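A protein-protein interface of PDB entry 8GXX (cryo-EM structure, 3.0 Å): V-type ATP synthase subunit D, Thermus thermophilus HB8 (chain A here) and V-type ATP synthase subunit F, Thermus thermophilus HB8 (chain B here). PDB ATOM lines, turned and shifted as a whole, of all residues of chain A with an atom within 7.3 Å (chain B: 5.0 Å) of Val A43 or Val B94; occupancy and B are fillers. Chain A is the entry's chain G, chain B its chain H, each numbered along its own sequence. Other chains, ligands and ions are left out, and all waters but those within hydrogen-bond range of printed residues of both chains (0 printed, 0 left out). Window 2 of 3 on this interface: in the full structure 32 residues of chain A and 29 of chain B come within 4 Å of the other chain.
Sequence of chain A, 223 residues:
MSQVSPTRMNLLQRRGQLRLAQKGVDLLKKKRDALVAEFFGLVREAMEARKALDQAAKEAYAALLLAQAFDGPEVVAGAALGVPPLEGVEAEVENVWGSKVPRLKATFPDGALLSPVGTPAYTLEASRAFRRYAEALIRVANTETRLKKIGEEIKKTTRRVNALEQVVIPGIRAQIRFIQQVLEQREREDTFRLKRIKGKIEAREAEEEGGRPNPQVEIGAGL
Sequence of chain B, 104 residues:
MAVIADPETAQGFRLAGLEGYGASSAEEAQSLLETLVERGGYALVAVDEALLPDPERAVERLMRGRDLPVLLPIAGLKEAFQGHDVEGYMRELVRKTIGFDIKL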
ATOM      1  N   GLU A  38      -2.109 -20.007  30.869  1.00  0.00           N
ATOM      2  CA  GLU A  38      -3.486 -19.556  30.681  1.00  0.00           C
ATOM      3  C   GLU A  38      -4.371 -20.674  30.141  1.00  0.00           C
ATOM      4  O   GLU A  38      -5.533 -20.819  30.552  1.00  0.00           O
ATOM      5  CB  GLU A  38      -3.510 -18.357  29.737  1.00  0.00           C
ATOM      6  CG  GLU A  38      -4.791 -18.223  28.939  1.00  0.00           C
ATOM      7  CD  GLU A  38      -4.877 -16.907  28.192  1.00  0.00           C
ATOM      8  OE1 GLU A  38      -3.903 -16.127  28.243  1.00  0.00           O
ATOM      9  OE2 GLU A  38      -5.919 -16.653  27.552  1.00  0.00           O
ATOM     10  N   PHE A  39      -3.835 -21.467  29.217  1.00  0.00           N
ATOM     11  CA  PHE A  39      -4.635 -22.457  28.511  1.00  0.00           C
ATOM     12  C   PHE A  39      -5.222 -23.473  29.470  1.00  0.00           C
ATOM     13  O   PHE A  39      -6.391 -23.850  29.345  1.00  0.00           O
ATOM     14  CB  PHE A  39      -3.764 -23.146  27.461  1.00  0.00           C
ATOM     15  CG  PHE A  39      -4.404 -24.330  26.802  1.00  0.00           C
ATOM     16  CD1 PHE A  39      -4.397 -25.563  27.415  1.00  0.00           C
ATOM     17  CD2 PHE A  39      -4.964 -24.218  25.549  1.00  0.00           C
ATOM     18  CE1 PHE A  39      -4.966 -26.650  26.809  1.00  0.00           C
ATOM     19  CE2 PHE A  39      -5.533 -25.307  24.937  1.00  0.00           C
ATOM     20  CZ  PHE A  39      -5.535 -26.521  25.564  1.00  0.00           C
ATOM     21  N   PHE A  40      -4.424 -23.952  30.419  1.00  0.00           N
ATOM     22  CA  PHE A  40      -4.931 -24.984  31.318  1.00  0.00           C
ATOM     23  C   PHE A  40      -6.052 -24.453  32.198  1.00  0.00           C
ATOM     24  O   PHE A  40      -7.069 -25.130  32.397  1.00  0.00           O
ATOM     25  CB  PHE A  40      -3.806 -25.536  32.185  1.00  0.00           C
ATOM     26  CG  PHE A  40      -2.936 -26.541  31.500  1.00  0.00           C
ATOM     27  CD1 PHE A  40      -3.220 -27.001  30.229  1.00  0.00           C
ATOM     28  CD2 PHE A  40      -1.823 -27.032  32.145  1.00  0.00           C
ATOM     29  CE1 PHE A  40      -2.405 -27.931  29.616  1.00  0.00           C
ATOM     30  CE2 PHE A  40      -1.007 -27.955  31.543  1.00  0.00           C
ATOM     31  CZ  PHE A  40      -1.296 -28.408  30.275  1.00  0.00           C
ATOM     32  N   GLY A  41      -5.876 -23.265  32.766  1.00  0.00           N
ATOM     33  CA  GLY A  41      -6.948 -22.688  33.554  1.00  0.00           C
ATOM     34  C   GLY A  41      -8.214 -22.545  32.739  1.00  0.00           C
ATOM     35  O   GLY A  41      -9.317 -22.832  33.216  1.00  0.00           O
ATOM     36  N   LEU A  42      -8.073 -22.125  31.488  1.00  0.00           N
ATOM     37  CA  LEU A  42      -9.253 -21.988  30.654  1.00  0.00           C
ATOM     38  C   LEU A  42      -9.860 -23.348  30.324  1.00  0.00           C
ATOM     39  O   LEU A  42     -11.073 -23.446  30.116  1.00  0.00           O
ATOM     40  CB  LEU A  42      -8.889 -21.209  29.395  1.00  0.00           C
ATOM     41  CG  LEU A  42     -10.013 -20.452  28.696  1.00  0.00           C
ATOM     42  CD1 LEU A  42     -10.704 -19.478  29.640  1.00  0.00           C
ATOM     43  CD2 LEU A  42      -9.457 -19.717  27.505  1.00  0.00           C
ATOM     44  N   VAL A  43      -9.049 -24.405  30.281  1.00  0.00           N
ATOM     45  CA  VAL A  43      -9.587 -25.745  30.054  1.00  0.00           C
ATOM     46  C   VAL A  43     -10.395 -26.208  31.257  1.00  0.00           C
ATOM     47  O   VAL A  43     -11.440 -26.850  31.113  1.00  0.00           O
ATOM     48  CB  VAL A  43      -8.455 -26.732  29.730  1.00  0.00           C
ATOM     49  CG1 VAL A  43      -8.940 -28.164  29.888  1.00  0.00           C
ATOM     50  CG2 VAL A  43      -7.946 -26.506  28.327  1.00  0.00           C
ATOM     51  N   ARG A  44      -9.924 -25.902  32.461  1.00  0.00           N
ATOM     52  CA  ARG A  44     -10.746 -26.151  33.642  1.00  0.00           C
ATOM     53  C   ARG A  44     -12.050 -25.367  33.567  1.00  0.00           C
ATOM     54  O   ARG A  44     -13.122 -25.883  33.910  1.00  0.00           O
ATOM     55  CB  ARG A  44      -9.984 -25.783  34.914  1.00  0.00           C
ATOM     56  CG  ARG A  44      -8.763 -26.637  35.164  1.00  0.00           C
ATOM     57  CD  ARG A  44      -8.028 -26.218  36.421  1.00  0.00           C
ATOM     58  NE  ARG A  44      -6.854 -27.052  36.651  1.00  0.00           N
ATOM     59  CZ  ARG A  44      -6.013 -26.910  37.666  1.00  0.00           C
ATOM     60  NH1 ARG A  44      -6.182 -25.966  38.578  1.00  0.00           N
ATOM     61  NH2 ARG A  44      -4.976 -27.736  37.768  1.00  0.00           N
ATOM     62  N   GLU A  45     -11.976 -24.108  33.140  1.00  0.00           N
ATOM     63  CA  GLU A  45     -13.191 -23.314  33.005  1.00  0.00           C
ATOM     64  C   GLU A  45     -14.156 -23.963  32.026  1.00  0.00           C
ATOM     65  O   GLU A  45     -15.367 -24.003  32.267  1.00  0.00           O
ATOM     66  CB  GLU A  45     -12.848 -21.897  32.553  1.00  0.00           C
ATOM     67  CG  GLU A  45     -14.058 -21.010  32.310  1.00  0.00           C
ATOM     68  CD  GLU A  45     -14.877 -20.785  33.565  1.00  0.00           C
ATOM     69  OE1 GLU A  45     -14.367 -21.068  34.670  1.00  0.00           O
ATOM     70  OE2 GLU A  45     -16.032 -20.324  33.450  1.00  0.00           O
ATOM     71  N   ALA A  46     -13.639 -24.457  30.902  1.00  0.00           N
ATOM     72  CA  ALA A  46     -14.488 -25.142  29.938  1.00  0.00           C
ATOM     73  C   ALA A  46     -15.074 -26.410  30.531  1.00  0.00           C
ATOM     74  O   ALA A  46     -16.210 -26.767  30.223  1.00  0.00           O
ATOM     75  CB  ALA A  46     -13.701 -25.460  28.671  1.00  0.00           C
ATOM     76  N   MET A  47     -14.317 -27.106  31.374  1.00  0.00           N
ATOM     77  CA  MET A  47     -14.860 -28.275  32.057  1.00  0.00           C
ATOM     78  C   MET A  47     -16.052 -27.888  32.922  1.00  0.00           C
ATOM     79  O   MET A  47     -17.099 -28.549  32.900  1.00  0.00           O
ATOM     80  CB  MET A  47     -13.770 -28.931  32.903  1.00  0.00           C
ATOM     81  CG  MET A  47     -14.246 -30.087  33.766  1.00  0.00           C
ATOM     82  SD  MET A  47     -12.922 -30.814  34.751  1.00  0.00           S
ATOM     83  CE  MET A  47     -12.524 -29.457  35.850  1.00  0.00           C
ATOM     84  N   GLU A  48     -15.909 -26.810  33.695  1.00  0.00           N
ATOM     85  CA  GLU A  48     -17.018 -26.362  34.530  1.00  0.00           C
ATOM     86  C   GLU A  48     -18.213 -25.969  33.675  1.00  0.00           C
ATOM     87  O   GLU A  48     -19.357 -26.316  33.988  1.00  0.00           O
ATOM     88  CB  GLU A  48     -16.594 -25.184  35.406  1.00  0.00           C
ATOM     89  CG  GLU A  48     -15.335 -25.417  36.226  1.00  0.00           C
ATOM     90  CD  GLU A  48     -15.426 -26.633  37.126  1.00  0.00           C
ATOM     91  OE1 GLU A  48     -16.555 -27.057  37.448  1.00  0.00           O
ATOM     92  OE2 GLU A  48     -14.365 -27.167  37.512  1.00  0.00           O
ATOM     93  N   ALA A  49     -17.969 -25.228  32.600  1.00  0.00           N
ATOM     94  CA  ALA A  49     -19.068 -24.810  31.742  1.00  0.00           C
ATOM     95  C   ALA A  49     -19.763 -26.018  31.138  1.00  0.00           C
ATOM     96  O   ALA A  49     -20.994 -26.061  31.055  1.00  0.00           O
ATOM     97  CB  ALA A  49     -18.556 -23.877  30.646  1.00  0.00           C
ATOM     98  N   THR A 143     -16.292 -20.198  25.749  1.00  0.00           N
ATOM     99  CA  THR A 143     -15.080 -20.740  26.359  1.00  0.00           C
ATOM    100  C   THR A 143     -14.358 -21.694  25.412  1.00  0.00           C
ATOM    101  O   THR A 143     -13.122 -21.677  25.329  1.00  0.00           O
ATOM    102  CB  THR A 143     -15.404 -21.426  27.685  1.00  0.00           C
ATOM    103  OG1 THR A 143     -14.188 -21.782  28.350  1.00  0.00           O
ATOM    104  CG2 THR A 143     -16.244 -22.673  27.479  1.00  0.00           C
ATOM    105  N   LEU A 147     -10.493 -21.337  23.993  1.00  0.00           N
ATOM    106  CA  LEU A 147      -9.496 -22.401  24.034  1.00  0.00           C
ATOM    107  C   LEU A 147      -8.910 -22.651  22.657  1.00  0.00           C
ATOM    108  O   LEU A 147      -7.699 -22.826  22.504  1.00  0.00           O
ATOM    109  CB  LEU A 147     -10.106 -23.698  24.556  1.00  0.00           C
ATOM    110  CG  LEU A 147     -10.574 -23.757  25.998  1.00  0.00           C
ATOM    111  CD1 LEU A 147     -10.912 -25.192  26.364  1.00  0.00           C
ATOM    112  CD2 LEU A 147      -9.508 -23.216  26.887  1.00  0.00           C
ATOM    113  N   MET B  90     -13.270 -33.822  27.326  1.00  0.00           N
ATOM    114  CA  MET B  90     -12.250 -32.799  27.508  1.00  0.00           C
ATOM    115  C   MET B  90     -10.860 -33.354  27.231  1.00  0.00           C
ATOM    116  O   MET B  90     -10.007 -32.654  26.680  1.00  0.00           O
ATOM    117  CB  MET B  90     -12.324 -32.226  28.919  1.00  0.00           C
ATOM    118  CG  MET B  90     -11.580 -30.915  29.076  1.00  0.00           C
ATOM    119  SD  MET B  90     -12.255 -29.615  28.030  1.00  0.00           S
ATOM    120  CE  MET B  90     -13.820 -29.318  28.841  1.00  0.00           C
ATOM    121  N   ARG B  91     -10.608 -34.603  27.619  1.00  0.00           N
ATOM    122  CA  ARG B  91      -9.325 -35.217  27.302  1.00  0.00           C
ATOM    123  C   ARG B  91      -9.139 -35.316  25.795  1.00  0.00           C
ATOM    124  O   ARG B  91      -8.062 -35.010  25.266  1.00  0.00           O
ATOM    125  CB  ARG B  91      -9.235 -36.597  27.948  1.00  0.00           C
ATOM    126  CG  ARG B  91      -7.859 -37.236  27.855  1.00  0.00           C
ATOM    127  CD  ARG B  91      -7.818 -38.565  28.590  1.00  0.00           C
ATOM    128  NE  ARG B  91      -8.079 -38.410  30.016  1.00  0.00           N
ATOM    129  CZ  ARG B  91      -7.145 -38.213  30.939  1.00  0.00           C
ATOM    130  NH1 ARG B  91      -5.862 -38.144  30.623  1.00  0.00           N
ATOM    131  NH2 ARG B  91      -7.509 -38.082  32.211  1.00  0.00           N
ATOM    132  N   GLU B  92     -10.190 -35.721  25.085  1.00  0.00           N
ATOM    133  CA  GLU B  92     -10.118 -35.754  23.630  1.00  0.00           C
ATOM    134  C   GLU B  92      -9.845 -34.367  23.068  1.00  0.00           C
ATOM    135  O   GLU B  92      -9.052 -34.210  22.133  1.00  0.00           O
ATOM    136  CB  GLU B  92     -11.415 -36.319  23.053  1.00  0.00           C
ATOM    137  CG  GLU B  92     -11.427 -36.412  21.536  1.00  0.00           C
ATOM    138  CD  GLU B  92     -12.714 -37.009  21.000  1.00  0.00           C
ATOM    139  OE1 GLU B  92     -13.618 -37.301  21.809  1.00  0.00           O
ATOM    140  OE2 GLU B  92     -12.818 -37.186  19.768  1.00  0.00           O
ATOM    141  N   LEU B  93     -10.488 -33.347  23.626  1.00  0.00           N
ATOM    142  CA  LEU B  93     -10.316 -32.002  23.093  1.00  0.00           C
ATOM    143  C   LEU B  93      -8.906 -31.479  23.340  1.00  0.00           C
ATOM    144  O   LEU B  93      -8.335 -30.801  22.481  1.00  0.00           O
ATOM    145  CB  LEU B  93     -11.357 -31.067  23.707  1.00  0.00           C
ATOM    146  CG  LEU B  93     -11.380 -29.623  23.206  1.00  0.00           C
ATOM    147  CD1 LEU B  93     -11.199 -29.553  21.705  1.00  0.00           C
ATOM    148  CD2 LEU B  93     -12.686 -28.966  23.613  1.00  0.00           C
ATOM    149  N   VAL B  94      -8.327 -31.769  24.508  1.00  0.00           N
ATOM    150  CA  VAL B  94      -6.959 -31.327  24.762  1.00  0.00           C
ATOM    151  C   VAL B  94      -5.991 -32.066  23.848  1.00  0.00           C
ATOM    152  O   VAL B  94      -5.009 -31.489  23.367  1.00  0.00           O
ATOM    153  CB  VAL B  94      -6.581 -31.496  26.245  1.00  0.00           C
ATOM    154  CG1 VAL B  94      -7.479 -30.639  27.122  1.00  0.00           C
ATOM    155  CG2 VAL B  94      -6.648 -32.943  26.667  1.00  0.00           C
ATOM    156  N   ARG B  95      -6.249 -33.347  23.587  1.00  0.00           N
ATOM    157  CA  ARG B  95      -5.481 -34.043  22.564  1.00  0.00           C
ATOM    158  C   ARG B  95      -5.580 -33.302  21.237  1.00  0.00           C
ATOM    159  O   ARG B  95      -4.571 -33.068  20.562  1.00  0.00           O
ATOM    160  CB  ARG B  95      -5.984 -35.479  22.422  1.00  0.00           C
ATOM    161  CG  ARG B  95      -5.367 -36.273  21.276  1.00  0.00           C
ATOM    162  CD  ARG B  95      -6.221 -37.484  20.952  1.00  0.00           C
ATOM    163  NE  ARG B  95      -6.455 -38.316  22.125  1.00  0.00           N
ATOM    164  CZ  ARG B  95      -7.330 -39.312  22.176  1.00  0.00           C
ATOM    165  NH1 ARG B  95      -8.083 -39.625  21.134  1.00  0.00           N
ATOM    166  NH2 ARG B  95      -7.455 -40.007  23.303  1.00  0.00           N
ATOM    167  N   LYS B  96      -6.793 -32.915  20.855  1.00  0.00           N
ATOM    168  CA  LYS B  96      -6.979 -32.223  19.586  1.00  0.00           C
ATOM    169  C   LYS B  96      -6.189 -30.922  19.545  1.00  0.00           C
ATOM    170  O   LYS B  96      -5.591 -30.580  18.519  1.00  0.00           O
ATOM    171  CB  LYS B  96      -8.464 -31.938  19.356  1.00  0.00           C
ATOM    172  CG  LYS B  96      -9.312 -33.155  19.031  1.00  0.00           C
ATOM    173  CD  LYS B  96     -10.783 -32.771  18.928  1.00  0.00           C
ATOM    174  CE  LYS B  96     -11.649 -33.948  18.512  1.00  0.00           C
ATOM    175  NZ  LYS B  96     -13.098 -33.606  18.538  1.00  0.00           N
ATOM    176  N   THR B  97      -6.186 -30.177  20.647  1.00  0.00           N
ATOM    177  CA  THR B  97      -5.644 -28.823  20.637  1.00  0.00           C
ATOM    178  C   THR B  97      -4.128 -28.797  20.803  1.00  0.00           C
ATOM    179  O   THR B  97      -3.426 -28.206  19.978  1.00  0.00           O
ATOM    180  CB  THR B  97      -6.302 -27.982  21.733  1.00  0.00           C
ATOM    181  OG1 THR B  97      -6.310 -28.713  22.963  1.00  0.00           O
ATOM    182  CG2 THR B  97      -7.727 -27.624  21.348  1.00  0.00           C
ATOM    183  N   ILE B  98      -3.606 -29.414  21.860  1.00  0.00           N
ATOM    184  CA  ILE B  98      -2.184 -29.351  22.166  1.00  0.00           C
ATOM    185  C   ILE B  98      -1.455 -30.604  21.708  1.00  0.00           C
ATOM    186  O   ILE B  98      -0.223 -30.635  21.711  1.00  0.00           O
ATOM    187  CB  ILE B  98      -1.958 -29.082  23.664  1.00  0.00           C
ATOM    188  CG1 ILE B  98      -2.386 -27.640  23.972  1.00  0.00           C
ATOM    189  CG2 ILE B  98      -0.505 -29.342  24.062  1.00  0.00           C
ATOM    190  CD1 ILE B  98      -2.109 -27.166  25.384  1.00  0.00           C
ATOM    191  N   GLY B  99      -2.182 -31.631  21.291  1.00  0.00           N
ATOM    192  CA  GLY B  99      -1.558 -32.770  20.651  1.00  0.00           C
ATOM    193  C   GLY B  99      -0.921 -33.755  21.605  1.00  0.00           C
ATOM    194  O   GLY B  99      -0.694 -34.911  21.240  1.00  0.00           O
ATOM    195  N   PHE B 100      -0.621 -33.320  22.826  1.00  0.00           N
ATOM    196  CA  PHE B 100       0.054 -34.202  23.770  1.00  0.00           C
ATOM    197  C   PHE B 100      -0.886 -35.237  24.365  1.00  0.00           C
ATOM    198  O   PHE B 100      -0.447 -36.341  24.694  1.00  0.00           O
ATOM    199  CB  PHE B 100       0.699 -33.387  24.894  1.00  0.00           C
ATOM    200  CG  PHE B 100       2.100 -32.915  24.593  1.00  0.00           C
ATOM    201  CD1 PHE B 100       2.645 -33.030  23.324  1.00  0.00           C
ATOM    202  CD2 PHE B 100       2.876 -32.361  25.597  1.00  0.00           C
ATOM    203  CE1 PHE B 100       3.926 -32.598  23.063  1.00  0.00           C
ATOM    204  CE2 PHE B 100       4.160 -31.926  25.339  1.00  0.00           C
ATOM    205  CZ  PHE B 100       4.684 -32.044  24.070  1.00  0.00           C
ATOM    206  N   ASP B 101      -2.162 -34.908  24.522  1.00  0.00           N
ATOM    207  CA  ASP B 101      -3.103 -35.804  25.182  1.00  0.00           C
ATOM    208  C   ASP B 101      -2.560 -36.219  26.544  1.00  0.00           C
ATOM    209  O   ASP B 101      -2.490 -37.401  26.888  1.00  0.00           O
ATOM    210  CB  ASP B 101      -3.396 -37.027  24.313  1.00  0.00           C
ATOM    211  CG  ASP B 101      -4.521 -37.881  24.865  1.00  0.00           C
ATOM    212  OD1 ASP B 101      -5.110 -37.499  25.899  1.00  0.00           O
ATOM    213  OD2 ASP B 101      -4.821 -38.933  24.262  1.00  0.00           O
ATOM    214  N   ILE B 102      -2.150 -35.224  27.320  1.00  0.00           N
ATOM    215  CA  ILE B 102      -1.526 -35.439  28.615  1.00  0.00           C
ATOM    216  C   ILE B 102      -2.342 -34.709  29.668  1.00  0.00           C
ATOM    217  O   ILE B 102      -2.672 -33.530  29.499  1.00  0.00           O
ATOM    218  CB  ILE B 102      -0.062 -34.966  28.622  1.00  0.00           C
ATOM    219  CG1 ILE B 102       0.786 -35.899  27.756  1.00  0.00           C
ATOM    220  CG2 ILE B 102       0.470 -34.918  30.043  1.00  0.00           C
ATOM    221  CD1 ILE B 102       2.212 -35.443  27.570  1.00  0.00           C
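The backbone carbonyl oxygen (O) of Leu B93 sits at hydrogen-bond distance from the side-chain hydroxyl (OG1) of Thr B97 (2.9 Å). The backbone carbonyl oxygen (O) of Val B94 is in hydrogen-bond range of the side-chain hydroxyl (OG1) of Thr B97.
Of the printed residues of chain B, Val A43 touches Met B90 (3.9 Å) and Val B94 (3.99 Å). Of the printed residues of chain A, Val B94 touches Val A43. Printed residues of chain A within 4 Å of Ile B98: Phe A39 (3.2 Å). Of the printed residues of chain B, Ala A46 touches Met B90 (3.6 Å). The nearest printed residue of chain B that does not touch Val A43 is Thr B97 (6.0 Å). The nearest printed residue of chain A that does not touch Ile B98 is Phe A40 (4.3 Å).
Among the printed residues, merely in contact across the chains: Phe A39 with Thr B97 (3.5 Å), Phe A39 with Ile B98 (3.2 Å), Val A43 with Met B90 (3.9 Å), Val A43 with Val B94 (3.99 Å), Ala A46 with Met B90 (3.6 Å) and Met A47 with Met B90 (3.4 Å).
Printed residues of chain A that touch a printed residue of chain B: Phe A39, Val A43, Ala A46 and Met A47. Among the printed residues, no Asp or Glu carboxylate lies within 4 Å of a Lys or Arg side-chain nitrogen of the other chain.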
